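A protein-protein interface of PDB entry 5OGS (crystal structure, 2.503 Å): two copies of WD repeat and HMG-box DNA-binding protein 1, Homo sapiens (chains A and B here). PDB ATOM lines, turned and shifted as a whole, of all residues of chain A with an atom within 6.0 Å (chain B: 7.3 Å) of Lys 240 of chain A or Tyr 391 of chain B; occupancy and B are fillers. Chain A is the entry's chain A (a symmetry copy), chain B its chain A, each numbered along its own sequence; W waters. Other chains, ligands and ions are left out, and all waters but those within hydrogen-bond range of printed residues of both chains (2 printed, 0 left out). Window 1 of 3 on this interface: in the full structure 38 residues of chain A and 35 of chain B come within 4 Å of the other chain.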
ATOM      1  N   PRO A 206      -5.629 -20.931   5.890  1.00  0.00           N
ATOM      2  CA  PRO A 206      -4.831 -22.164   5.893  1.00  0.00           C
ATOM      3  C   PRO A 206      -4.314 -22.512   4.505  1.00  0.00           C
ATOM      4  O   PRO A 206      -4.665 -21.897   3.494  1.00  0.00           O
ATOM      5  CB  PRO A 206      -5.814 -23.221   6.407  1.00  0.00           C
ATOM      6  CG  PRO A 206      -6.799 -22.450   7.215  1.00  0.00           C
ATOM      7  CD  PRO A 206      -6.951 -21.132   6.509  1.00  0.00           C
ATOM      8  N   ARG A 231     -16.154 -17.629   6.624  1.00  0.00           N
ATOM      9  CA  ARG A 231     -15.461 -17.225   7.837  1.00  0.00           C
ATOM     10  C   ARG A 231     -15.937 -15.841   8.247  1.00  0.00           C
ATOM     11  O   ARG A 231     -15.927 -14.910   7.435  1.00  0.00           O
ATOM     12  CB  ARG A 231     -13.947 -17.232   7.622  1.00  0.00           C
ATOM     13  CG  ARG A 231     -13.411 -18.569   7.139  1.00  0.00           C
ATOM     14  CD  ARG A 231     -11.910 -18.520   6.918  1.00  0.00           C
ATOM     15  NE  ARG A 231     -11.372 -19.838   6.600  1.00  0.00           N
ATOM     16  CZ  ARG A 231     -10.969 -20.716   7.511  1.00  0.00           C
ATOM     17  NH1 ARG A 231     -11.044 -20.415   8.800  1.00  0.00           N
ATOM     18  NH2 ARG A 231     -10.491 -21.896   7.136  1.00  0.00           N
ATOM     19  N   LEU A 232     -16.362 -15.712   9.499  1.00  0.00           N
ATOM     20  CA  LEU A 232     -16.823 -14.446  10.044  1.00  0.00           C
ATOM     21  C   LEU A 232     -15.728 -13.816  10.895  1.00  0.00           C
ATOM     22  O   LEU A 232     -15.038 -14.505  11.653  1.00  0.00           O
ATOM     23  CB  LEU A 232     -18.091 -14.638  10.878  1.00  0.00           C
ATOM     24  CG  LEU A 232     -19.349 -15.017  10.096  1.00  0.00           C
ATOM     25  CD1 LEU A 232     -20.505 -15.293  11.041  1.00  0.00           C
ATOM     26  CD2 LEU A 232     -19.712 -13.918   9.110  1.00  0.00           C
ATOM     27  N   PHE A 233     -15.572 -12.504  10.760  1.00  0.00           N
ATOM     28  CA  PHE A 233     -14.588 -11.745  11.515  1.00  0.00           C
ATOM     29  C   PHE A 233     -15.243 -10.488  12.063  1.00  0.00           C
ATOM     30  O   PHE A 233     -16.085  -9.880  11.396  1.00  0.00           O
ATOM     31  CB  PHE A 233     -13.382 -11.347  10.649  1.00  0.00           C
ATOM     32  CG  PHE A 233     -12.740 -12.496   9.923  1.00  0.00           C
ATOM     33  CD1 PHE A 233     -13.236 -12.928   8.703  1.00  0.00           C
ATOM     34  CD2 PHE A 233     -11.626 -13.129  10.449  1.00  0.00           C
ATOM     35  CE1 PHE A 233     -12.643 -13.980   8.029  1.00  0.00           C
ATOM     36  CE2 PHE A 233     -11.028 -14.182   9.779  1.00  0.00           C
ATOM     37  CZ  PHE A 233     -11.537 -14.608   8.568  1.00  0.00           C
ATOM     38  N   THR A 234     -14.863 -10.103  13.275  1.00  0.00           N
ATOM     39  CA  THR A 234     -15.217  -8.774  13.739  1.00  0.00           C
ATOM     40  C   THR A 234     -14.387  -7.739  12.987  1.00  0.00           C
ATOM     41  O   THR A 234     -13.331  -8.042  12.424  1.00  0.00           O
ATOM     42  CB  THR A 234     -14.990  -8.639  15.244  1.00  0.00           C
ATOM     43  OG1 THR A 234     -13.586  -8.683  15.524  1.00  0.00           O
ATOM     44  CG2 THR A 234     -15.693  -9.763  15.995  1.00  0.00           C
ATOM     45  N   VAL A 238     -11.238 -10.203  15.309  1.00  0.00           N
ATOM     46  CA  VAL A 238     -11.554 -11.434  16.028  1.00  0.00           C
ATOM     47  C   VAL A 238     -12.234 -12.406  15.075  1.00  0.00           C
ATOM     48  O   VAL A 238     -13.158 -12.033  14.344  1.00  0.00           O
ATOM     49  CB  VAL A 238     -12.444 -11.143  17.247  1.00  0.00           C
ATOM     50  CG1 VAL A 238     -12.727 -12.424  18.017  1.00  0.00           C
ATOM     51  CG2 VAL A 238     -11.791 -10.110  18.142  1.00  0.00           C
ATOM     52  N   GLN A 239     -11.777 -13.657  15.079  1.00  0.00           N
ATOM     53  CA  GLN A 239     -12.406 -14.700  14.278  1.00  0.00           C
ATOM     54  C   GLN A 239     -13.695 -15.150  14.955  1.00  0.00           C
ATOM     55  O   GLN A 239     -13.675 -15.590  16.110  1.00  0.00           O
ATOM     56  CB  GLN A 239     -11.458 -15.883  14.093  1.00  0.00           C
ATOM     57  CG  GLN A 239     -10.179 -15.554  13.344  1.00  0.00           C
ATOM     58  CD  GLN A 239      -9.334 -16.784  13.072  1.00  0.00           C
ATOM     59  OE1 GLN A 239      -8.367 -17.056  13.783  1.00  0.00           O
ATOM     60  NE2 GLN A 239      -9.696 -17.533  12.040  1.00  0.00           N
ATOM     61  N   LYS A 240     -14.814 -15.038  14.241  1.00  0.00           N
ATOM     62  CA  LYS A 240     -16.102 -15.455  14.781  1.00  0.00           C
ATOM     63  C   LYS A 240     -16.446 -16.866  14.321  1.00  0.00           C
ATOM     64  O   LYS A 240     -15.559 -17.718  14.202  1.00  0.00           O
ATOM     65  CB  LYS A 240     -17.202 -14.473  14.371  1.00  0.00           C
ATOM     66  CG  LYS A 240     -17.059 -13.087  14.978  1.00  0.00           C
ATOM     67  CD  LYS A 240     -17.203 -13.130  16.490  1.00  0.00           C
ATOM     68  CE  LYS A 240     -18.299 -12.191  16.966  1.00  0.00           C
ATOM     69  NZ  LYS A 240     -19.618 -12.531  16.365  1.00  0.00           N
ATOM     70  N   GLU A 241     -17.724 -17.121  14.051  1.00  0.00           N
ATOM     71  CA  GLU A 241     -18.157 -18.461  13.686  1.00  0.00           C
ATOM     72  C   GLU A 241     -17.737 -18.805  12.259  1.00  0.00           C
ATOM     73  O   GLU A 241     -17.430 -17.936  11.438  1.00  0.00           O
ATOM     74  CB  GLU A 241     -19.674 -18.595  13.825  1.00  0.00           C
ATOM     75  CG  GLU A 241     -20.201 -18.336  15.226  1.00  0.00           C
ATOM     76  CD  GLU A 241     -20.641 -16.900  15.428  1.00  0.00           C
ATOM     77  OE1 GLU A 241     -21.600 -16.675  16.197  1.00  0.00           O
ATOM     78  OE2 GLU A 241     -20.037 -15.996  14.814  1.00  0.00           O
ATOM     79  N   VAL A 242     -17.725 -20.106  11.974  1.00  0.00           N
ATOM     80  CA  VAL A 242     -17.416 -20.637  10.651  1.00  0.00           C
ATOM     81  C   VAL A 242     -18.437 -21.719  10.326  1.00  0.00           C
ATOM     82  O   VAL A 242     -18.774 -22.542  11.183  1.00  0.00           O
ATOM     83  CB  VAL A 242     -15.978 -21.202  10.585  1.00  0.00           C
ATOM     84  CG1 VAL A 242     -15.697 -21.800   9.216  1.00  0.00           C
ATOM     85  CG2 VAL A 242     -14.958 -20.124  10.914  1.00  0.00           C
ATOM     86  N   LEU A 282     -27.078 -12.045  11.771  1.00  0.00           N
ATOM     87  CA  LEU A 282     -25.998 -12.419  12.675  1.00  0.00           C
ATOM     88  C   LEU A 282     -26.012 -11.620  13.974  1.00  0.00           C
ATOM     89  O   LEU A 282     -24.949 -11.352  14.547  1.00  0.00           O
ATOM     90  CB  LEU A 282     -24.651 -12.266  11.968  1.00  0.00           C
ATOM     91  CG  LEU A 282     -24.529 -13.001  10.631  1.00  0.00           C
ATOM     92  CD1 LEU A 282     -23.157 -12.784  10.015  1.00  0.00           C
ATOM     93  CD2 LEU A 282     -24.818 -14.484  10.804  1.00  0.00           C
ATOM     94  N   LYS A 286     -29.063 -15.729  16.329  1.00  0.00           N
ATOM     95  CA  LYS A 286     -28.747 -16.085  14.951  1.00  0.00           C
ATOM     96  C   LYS A 286     -29.959 -16.695  14.260  1.00  0.00           C
ATOM     97  O   LYS A 286     -30.619 -17.586  14.804  1.00  0.00           O
ATOM     98  CB  LYS A 286     -27.571 -17.058  14.912  1.00  0.00           C
ATOM     99  CG  LYS A 286     -26.220 -16.393  14.696  1.00  0.00           C
ATOM    100  CD  LYS A 286     -25.785 -15.576  15.897  1.00  0.00           C
ATOM    101  CE  LYS A 286     -24.449 -14.893  15.640  1.00  0.00           C
ATOM    102  NZ  LYS A 286     -24.022 -14.057  16.793  1.00  0.00           N
ATOM    103  N   THR B 335     -21.167 -26.811  10.611  1.00  0.00           N
ATOM    104  CA  THR B 335     -19.838 -26.327  10.941  1.00  0.00           C
ATOM    105  C   THR B 335     -18.843 -27.475  10.952  1.00  0.00           C
ATOM    106  O   THR B 335     -19.107 -28.509  11.580  1.00  0.00           O
ATOM    107  CB  THR B 335     -19.846 -25.635  12.310  1.00  0.00           C
ATOM    108  OG1 THR B 335     -20.642 -24.445  12.243  1.00  0.00           O
ATOM    109  CG2 THR B 335     -18.430 -25.283  12.751  1.00  0.00           C
ATOM    110  N   PRO B 336     -17.703 -27.342  10.271  1.00  0.00           N
ATOM    111  CA  PRO B 336     -16.671 -28.385  10.350  1.00  0.00           C
ATOM    112  C   PRO B 336     -16.045 -28.413  11.738  1.00  0.00           C
ATOM    113  O   PRO B 336     -15.626 -27.381  12.265  1.00  0.00           O
ATOM    114  CB  PRO B 336     -15.652 -27.964   9.282  1.00  0.00           C
ATOM    115  CG  PRO B 336     -16.367 -26.965   8.425  1.00  0.00           C
ATOM    116  CD  PRO B 336     -17.335 -26.276   9.328  1.00  0.00           C
ATOM    117  N   LYS B 388     -11.064 -30.233  16.056  1.00  0.00           N
ATOM    118  CA  LYS B 388     -10.351 -28.993  15.764  1.00  0.00           C
ATOM    119  C   LYS B 388     -11.100 -28.267  14.658  1.00  0.00           C
ATOM    120  O   LYS B 388     -11.168 -28.760  13.528  1.00  0.00           O
ATOM    121  CB  LYS B 388      -8.906 -29.270  15.359  1.00  0.00           C
ATOM    122  CG  LYS B 388      -8.209 -28.085  14.709  1.00  0.00           C
ATOM    123  CD  LYS B 388      -6.897 -28.501  14.063  1.00  0.00           C
ATOM    124  CE  LYS B 388      -6.357 -27.403  13.160  1.00  0.00           C
ATOM    125  NZ  LYS B 388      -5.087 -27.799  12.490  1.00  0.00           N
ATOM    126  N   LEU B 389     -11.662 -27.108  14.981  1.00  0.00           N
ATOM    127  CA  LEU B 389     -12.347 -26.314  13.974  1.00  0.00           C
ATOM    128  C   LEU B 389     -11.320 -25.637  13.066  1.00  0.00           C
ATOM    129  O   LEU B 389     -10.252 -25.229  13.533  1.00  0.00           O
ATOM    130  CB  LEU B 389     -13.252 -25.273  14.631  1.00  0.00           C
ATOM    131  CG  LEU B 389     -14.660 -25.724  15.046  1.00  0.00           C
ATOM    132  CD1 LEU B 389     -14.630 -26.776  16.149  1.00  0.00           C
ATOM    133  CD2 LEU B 389     -15.517 -24.534  15.464  1.00  0.00           C
ATOM    134  N   PRO B 390     -11.608 -25.510  11.764  1.00  0.00           N
ATOM    135  CA  PRO B 390     -10.592 -25.023  10.801  1.00  0.00           C
ATOM    136  C   PRO B 390     -10.396 -23.513  10.859  1.00  0.00           C
ATOM    137  O   PRO B 390     -10.779 -22.754   9.961  1.00  0.00           O
ATOM    138  CB  PRO B 390     -11.169 -25.491   9.461  1.00  0.00           C
ATOM    139  CG  PRO B 390     -12.648 -25.421   9.667  1.00  0.00           C
ATOM    140  CD  PRO B 390     -12.887 -25.828  11.103  1.00  0.00           C
ATOM    141  N   TYR B 391      -9.768 -23.050  11.933  1.00  0.00           N
ATOM    142  CA  TYR B 391      -9.548 -21.624  12.123  1.00  0.00           C
ATOM    143  C   TYR B 391      -8.173 -21.209  11.608  1.00  0.00           C
ATOM    144  O   TYR B 391      -7.253 -22.021  11.481  1.00  0.00           O
ATOM    145  CB  TYR B 391      -9.707 -21.246  13.595  1.00  0.00           C
ATOM    146  CG  TYR B 391     -11.138 -20.944  13.965  1.00  0.00           C
ATOM    147  CD1 TYR B 391     -11.581 -19.634  14.086  1.00  0.00           C
ATOM    148  CD2 TYR B 391     -12.053 -21.968  14.166  1.00  0.00           C
ATOM    149  CE1 TYR B 391     -12.892 -19.353  14.413  1.00  0.00           C
ATOM    150  CE2 TYR B 391     -13.368 -21.696  14.492  1.00  0.00           C
ATOM    151  CZ  TYR B 391     -13.782 -20.387  14.614  1.00  0.00           C
ATOM    152  OH  TYR B 391     -15.088 -20.112  14.936  1.00  0.00           O
ATOM    153  N   CYS B 392      -8.051 -19.921  11.302  1.00  0.00           N
ATOM    154  CA  CYS B 392      -6.836 -19.382  10.711  1.00  0.00           C
ATOM    155  C   CYS B 392      -5.789 -19.087  11.776  1.00  0.00           C
ATOM    156  O   CYS B 392      -6.112 -18.727  12.913  1.00  0.00           O
ATOM    157  CB  CYS B 392      -7.144 -18.105   9.927  1.00  0.00           C
ATOM    158  SG  CYS B 392      -8.367 -18.300   8.614  1.00  0.00           S
ATOM    159  N   GLN B 393      -4.522 -19.238  11.388  1.00  0.00           N
ATOM    160  CA  GLN B 393      -3.373 -18.926  12.241  1.00  0.00           C
ATOM    161  C   GLN B 393      -3.501 -19.594  13.608  1.00  0.00           C
ATOM    162  O   GLN B 393      -3.283 -18.980  14.655  1.00  0.00           O
ATOM    163  CB  GLN B 393      -3.194 -17.414  12.381  1.00  0.00           C
ATOM    164  CG  GLN B 393      -2.939 -16.699  11.063  1.00  0.00           C
ATOM    165  CD  GLN B 393      -2.579 -15.239  11.251  1.00  0.00           C
ATOM    166  OE1 GLN B 393      -2.560 -14.732  12.373  1.00  0.00           O
ATOM    167  NE2 GLN B 393      -2.288 -14.554  10.152  1.00  0.00           N
ATOM    168  N   ILE B 394      -3.861 -20.880  13.588  1.00  0.00           N
ATOM    169  CA  ILE B 394      -4.081 -21.621  14.824  1.00  0.00           C
ATOM    170  C   ILE B 394      -2.794 -21.872  15.595  1.00  0.00           C
ATOM    171  O   ILE B 394      -2.850 -22.259  16.768  1.00  0.00           O
ATOM    172  CB  ILE B 394      -4.801 -22.950  14.514  1.00  0.00           C
ATOM    173  CG1 ILE B 394      -5.551 -23.456  15.748  1.00  0.00           C
ATOM    174  CG2 ILE B 394      -3.810 -23.992  14.017  1.00  0.00           C
ATOM    175  CD1 ILE B 394      -6.477 -24.614  15.468  1.00  0.00           C
ATOM    176  N   ALA B 395      -1.634 -21.654  14.973  1.00  0.00           N
ATOM    177  CA  ALA B 395      -0.371 -21.772  15.693  1.00  0.00           C
ATOM    178  C   ALA B 395      -0.129 -20.593  16.627  1.00  0.00           C
ATOM    179  O   ALA B 395       0.628 -20.731  17.594  1.00  0.00           O
ATOM    180  CB  ALA B 395       0.791 -21.904  14.709  1.00  0.00           C
ATOM    181  N   GLY B 399      -5.169 -17.261  17.531  1.00  0.00           N
ATOM    182  CA  GLY B 399      -5.922 -18.257  16.785  1.00  0.00           C
ATOM    183  C   GLY B 399      -6.202 -19.510  17.594  1.00  0.00           C
ATOM    184  O   GLY B 399      -7.264 -20.123  17.459  1.00  0.00           O
ATOM    185  N   GLN B 400      -5.253 -19.907  18.445  1.00  0.00           N
ATOM    186  CA  GLN B 400      -5.454 -21.084  19.284  1.00  0.00           C
ATOM    187  C   GLN B 400      -6.610 -20.875  20.254  1.00  0.00           C
ATOM    188  O   GLN B 400      -7.482 -21.740  20.397  1.00  0.00           O
ATOM    189  CB  GLN B 400      -4.168 -21.411  20.043  1.00  0.00           C
ATOM    190  CG  GLN B 400      -4.326 -22.487  21.105  1.00  0.00           C
ATOM    191  CD  GLN B 400      -3.072 -22.676  21.938  1.00  0.00           C
ATOM    192  OE1 GLN B 400      -2.017 -22.125  21.626  1.00  0.00           O
ATOM    193  NE2 GLN B 400      -3.185 -23.457  23.006  1.00  0.00           N
ATOM    194  N   GLU B 402      -9.027 -18.622  19.993  1.00  0.00           N
ATOM    195  CA  GLU B 402     -10.271 -18.424  19.257  1.00  0.00           C
ATOM    196  C   GLU B 402     -10.878 -19.755  18.833  1.00  0.00           C
ATOM    197  O   GLU B 402     -12.103 -19.924  18.858  1.00  0.00           O
ATOM    198  CB  GLU B 402     -10.027 -17.529  18.042  1.00  0.00           C
ATOM    199  CG  GLU B 402      -9.872 -16.057  18.384  1.00  0.00           C
ATOM    200  CD  GLU B 402      -9.404 -15.228  17.205  1.00  0.00           C
ATOM    201  OE1 GLU B 402      -8.735 -15.788  16.310  1.00  0.00           O
ATOM    202  OE2 GLU B 402      -9.706 -14.017  17.171  1.00  0.00           O
ATOM    203  N   GLU B 403     -10.036 -20.714  18.440  1.00  0.00           N
ATOM    204  CA  GLU B 403     -10.544 -22.041  18.107  1.00  0.00           C
ATOM    205  C   GLU B 403     -11.114 -22.734  19.339  1.00  0.00           C
ATOM    206  O   GLU B 403     -12.169 -23.374  19.264  1.00  0.00           O
ATOM    207  CB  GLU B 403      -9.437 -22.886  17.473  1.00  0.00           C
ATOM    208  CG  GLU B 403      -9.910 -24.200  16.854  1.00  0.00           C
ATOM    209  CD  GLU B 403     -10.081 -25.311  17.874  1.00  0.00           C
ATOM    210  OE1 GLU B 403      -9.401 -25.266  18.921  1.00  0.00           O
ATOM    211  OE2 GLU B 403     -10.899 -26.223  17.632  1.00  0.00           O
ATOM    212  N   GLN B 404     -10.431 -22.617  20.482  1.00  0.00           N
ATOM    213  CA  GLN B 404     -10.921 -23.249  21.703  1.00  0.00           C
ATOM    214  C   GLN B 404     -12.247 -22.645  22.142  1.00  0.00           C
ATOM    215  O   GLN B 404     -13.123 -23.355  22.651  1.00  0.00           O
ATOM    216  CB  GLN B 404      -9.885 -23.118  22.819  1.00  0.00           C
ATOM    217  CG  GLN B 404      -8.563 -23.809  22.543  1.00  0.00           C
ATOM    218  CD  GLN B 404      -7.587 -23.667  23.695  1.00  0.00           C
ATOM    219  OE1 GLN B 404      -6.382 -23.520  23.489  1.00  0.00           O
ATOM    220  NE2 GLN B 404      -8.103 -23.713  24.917  1.00  0.00           N
ATOM    221  N   PHE B 405     -12.412 -21.334  21.954  1.00  0.00           N
ATOM    222  CA  PHE B 405     -13.645 -20.674  22.369  1.00  0.00           C
ATOM    223  C   PHE B 405     -14.834 -21.161  21.551  1.00  0.00           C
ATOM    224  O   PHE B 405     -15.862 -21.561  22.110  1.00  0.00           O
ATOM    225  CB  PHE B 405     -13.490 -19.158  22.249  1.00  0.00           C
ATOM    226  CG  PHE B 405     -14.755 -18.398  22.529  1.00  0.00           C
ATOM    227  CD1 PHE B 405     -15.152 -18.149  23.832  1.00  0.00           C
ATOM    228  CD2 PHE B 405     -15.545 -17.930  21.492  1.00  0.00           C
ATOM    229  CE1 PHE B 405     -16.315 -17.451  24.095  1.00  0.00           C
ATOM    230  CE2 PHE B 405     -16.710 -17.232  21.749  1.00  0.00           C
ATOM    231  CZ  PHE B 405     -17.095 -16.992  23.053  1.00  0.00           C
ATOM    232  N   TRP B 406     -14.710 -21.140  20.223  1.00  0.00           N
ATOM    233  CA  TRP B 406     -15.842 -21.499  19.376  1.00  0.00           C
ATOM    234  C   TRP B 406     -16.095 -22.999  19.373  1.00  0.00           C
ATOM    235  O   TRP B 406     -17.233 -23.431  19.153  1.00  0.00           O
ATOM    236  CB  TRP B 406     -15.617 -20.982  17.957  1.00  0.00           C
ATOM    237  CG  TRP B 406     -15.696 -19.492  17.878  1.00  0.00           C
ATOM    238  CD1 TRP B 406     -14.681 -18.629  17.586  1.00  0.00           C
ATOM    239  CD2 TRP B 406     -16.853 -18.684  18.121  1.00  0.00           C
ATOM    240  NE1 TRP B 406     -15.138 -17.333  17.619  1.00  0.00           N
ATOM    241  CE2 TRP B 406     -16.468 -17.340  17.947  1.00  0.00           C
ATOM    242  CE3 TRP B 406     -18.179 -18.967  18.464  1.00  0.00           C
ATOM    243  CZ2 TRP B 406     -17.360 -16.282  18.104  1.00  0.00           C
ATOM    244  CZ3 TRP B 406     -19.064 -17.915  18.620  1.00  0.00           C
ATOM    245  CH2 TRP B 406     -18.651 -16.589  18.439  1.00  0.00           C
ATOM    246  N   ARG B 407     -15.060 -23.809  19.607  1.00  0.00           N
ATOM    247  CA  ARG B 407     -15.287 -25.235  19.803  1.00  0.00           C
ATOM    248  C   ARG B 407     -16.077 -25.483  21.083  1.00  0.00           C
ATOM    249  O   ARG B 407     -16.967 -26.343  21.116  1.00  0.00           O
ATOM    250  CB  ARG B 407     -13.954 -25.983  19.829  1.00  0.00           C
ATOM    251  CG  ARG B 407     -14.071 -27.456  20.188  1.00  0.00           C
ATOM    252  CD  ARG B 407     -12.873 -28.247  19.686  1.00  0.00           C
ATOM    253  NE  ARG B 407     -11.612 -27.562  19.955  1.00  0.00           N
ATOM    254  CZ  ARG B 407     -10.945 -27.647  21.101  1.00  0.00           C
ATOM    255  NH1 ARG B 407     -11.420 -28.387  22.096  1.00  0.00           N
ATOM    256  NH2 ARG B 407      -9.805 -26.989  21.257  1.00  0.00           N
ATOM    257  N   GLU B 459     -14.611  -5.535  21.554  1.00  0.00           N
ATOM    258  CA  GLU B 459     -15.321  -6.563  20.799  1.00  0.00           C
ATOM    259  C   GLU B 459     -15.359  -7.879  21.564  1.00  0.00           C
ATOM    260  O   GLU B 459     -16.387  -8.564  21.588  1.00  0.00           O
ATOM    261  CB  GLU B 459     -14.665  -6.763  19.434  1.00  0.00           C
ATOM    262  CG  GLU B 459     -14.792  -5.580  18.496  1.00  0.00           C
ATOM    263  CD  GLU B 459     -14.161  -5.854  17.149  1.00  0.00           C
ATOM    264  OE1 GLU B 459     -13.177  -6.621  17.101  1.00  0.00           O
ATOM    265  OE2 GLU B 459     -14.659  -5.318  16.137  1.00  0.00           O
ATOM    266  N   LEU B 463     -18.834 -10.357  24.071  1.00  0.00           N
ATOM    267  CA  LEU B 463     -19.150 -11.762  24.286  1.00  0.00           C
ATOM    268  C   LEU B 463     -19.103 -12.165  25.755  1.00  0.00           C
ATOM    269  O   LEU B 463     -19.425 -13.314  26.075  1.00  0.00           O
ATOM    270  CB  LEU B 463     -18.184 -12.641  23.485  1.00  0.00           C
ATOM    271  CG  LEU B 463     -18.151 -12.439  21.969  1.00  0.00           C
ATOM    272  CD1 LEU B 463     -16.957 -13.154  21.362  1.00  0.00           C
ATOM    273  CD2 LEU B 463     -19.439 -12.936  21.340  1.00  0.00           C
HETATM  274  O   HOH W   1     -11.735 -17.918  10.271  1.00  0.00           O
HETATM  275  O   HOH W   2     -17.565 -21.919  14.408  1.00  0.00           O
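The backbone carbonyl oxygen (O) of Pro 390 of chain B is in hydrogen-bond range of the guanidinium group (NH1) of Arg 231 of chain A, at 2.6 Å. The side-chain sulfur of Cys 392 of chain B lies within hydrogen-bond range of the guanidinium group of Arg 231 of chain A, 3.4 Å away. The side-chain hydroxyl (OH) of Tyr 391 of chain B sits at hydrogen-bond distance from the backbone carbonyl oxygen (O) of Lys 240 of chain A (2.5 Å). OE1 of Gln 239 of chain A lies close to OE1 of Glu 402 of chain B (2.9 Å). The indole nitrogen (NE1) of Trp 406 of chain B lies within hydrogen-bond range of the backbone carbonyl oxygen (O) of Gln 239 of chain A, at 2.7 Å. The side-chain hydroxyl of Thr 335 of chain B sits at hydrogen-bond distance from the backbone carbonyl oxygen of Val 242 of chain A, 2.9 Å away. The backbone carbonyl oxygen of Cys 392 of chain B sits close to the side-chain amide oxygen of Gln 239 of chain A, at 2.9 Å. The backbone carbonyl oxygen of Lys 240 of chain A sits at hydrogen-bond distance from the indole nitrogen of Trp 406 of chain B (3.5 Å). OG1 of Thr 234 of chain A lies within hydrogen-bond range of OE1 of Glu 459 of chain B, 2.6 Å away.
The backbone carbonyl oxygen of Leu 232 of chain A is in hydrogen-bond range of the backbone NH of Lys 240 of chain A (2.7 Å). OG1 of Thr 234 of chain A is in hydrogen-bond range of N of Val 238 of chain A (2.8 Å). The side-chain amino group of Lys 240 of chain A lies within salt-bridge range of the side-chain carboxylate of Glu 241 of chain A (3.8 Å). O of Glu 241 of chain A lies within hydrogen-bond range of N of Leu 232 of chain A (3.1 Å). The side-chain carboxylate (OE1) of Glu 241 of chain A lies within salt-bridge range of the side-chain amino group (NZ) of Lys 286 of chain A (3.6 Å).
SG of Cys 392 of chain B touches CD of Pro 206 of chain A (3.8 Å). Tyr 391 of chain B touches Arg 231 of chain A. OE2 of Glu 402 of chain B touches CA of Val 238 of chain A (3.4 Å). OE1 of Glu 459 of chain B touches CG2 of Val 238 of chain A, 3.9 Å away. Tyr 391 of chain B touches Gln 239 of chain A (CD1 to NE2, 3.5 Å). CA of Glu 241 of chain A touches OH of Tyr 391 of chain B, 3.7 Å away. Trp 406 of chain B touches Glu 241 of chain A. Tyr 391 of chain B touches Val 242 of chain A.
Printed residues of chain B within 4 Å of Gln 239 of chain A: Tyr 391 (3.5 Å), Cys 392 (2.9 Å), Glu 402 (2.9 Å) and Trp 406 (2.7 Å). Lys 240 of chain A touches two residues of chain B. Printed residues of chain A within 4 Å of Pro 390 of chain B: Arg 231 (2.6 Å). Of chain A, only Arg 231, Gln 239, Lys 240, Glu 241 and Val 242 come within 4 Å of Tyr 391 of chain B. Arg 407 of chain B touches none of the printed residues of chain A. The nearest printed residue of chain B that does not touch Thr 234 of chain A is Leu 463 of chain B (6.5 Å).
Of the 12 printed residues of chain A, 8 touch a printed residue of chain B. Of the 20 printed residues of chain B, 7 touch a printed residue of chain A. Printed residues of chain B that touch a printed residue of chain A: Thr 335, Pro 390, Tyr 391, Cys 392, Glu 402, Trp 406 and Glu 459. Hydrophobic or aromatic side chains of chain B that line the printed part of chain A: Tyr 391 and Trp 406. Among the printed residues, 17 pairs touch across the chains. Among the printed residues, no Asp or Glu carboxylate lies within 4 Å of a Lys or Arg side-chain nitrogen of the other chain.
No position is printed for both chains. Of the 17 pairs that touch across the chains among the printed residues, none has its exchanged pair printed and touching as well.
Water W1 lies within hydrogen-bond range of NE2 of Gln 239 of chain A (2.7 Å), NH1 of Arg 231 of chain A (3.0 Å) and SG of Cys 392 of chain B (3.8 Å). Water W2 lies within hydrogen-bond range of N of Val 242 of chain A (3.0 Å) and OH of Tyr 391 of chain B (3.1 Å).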
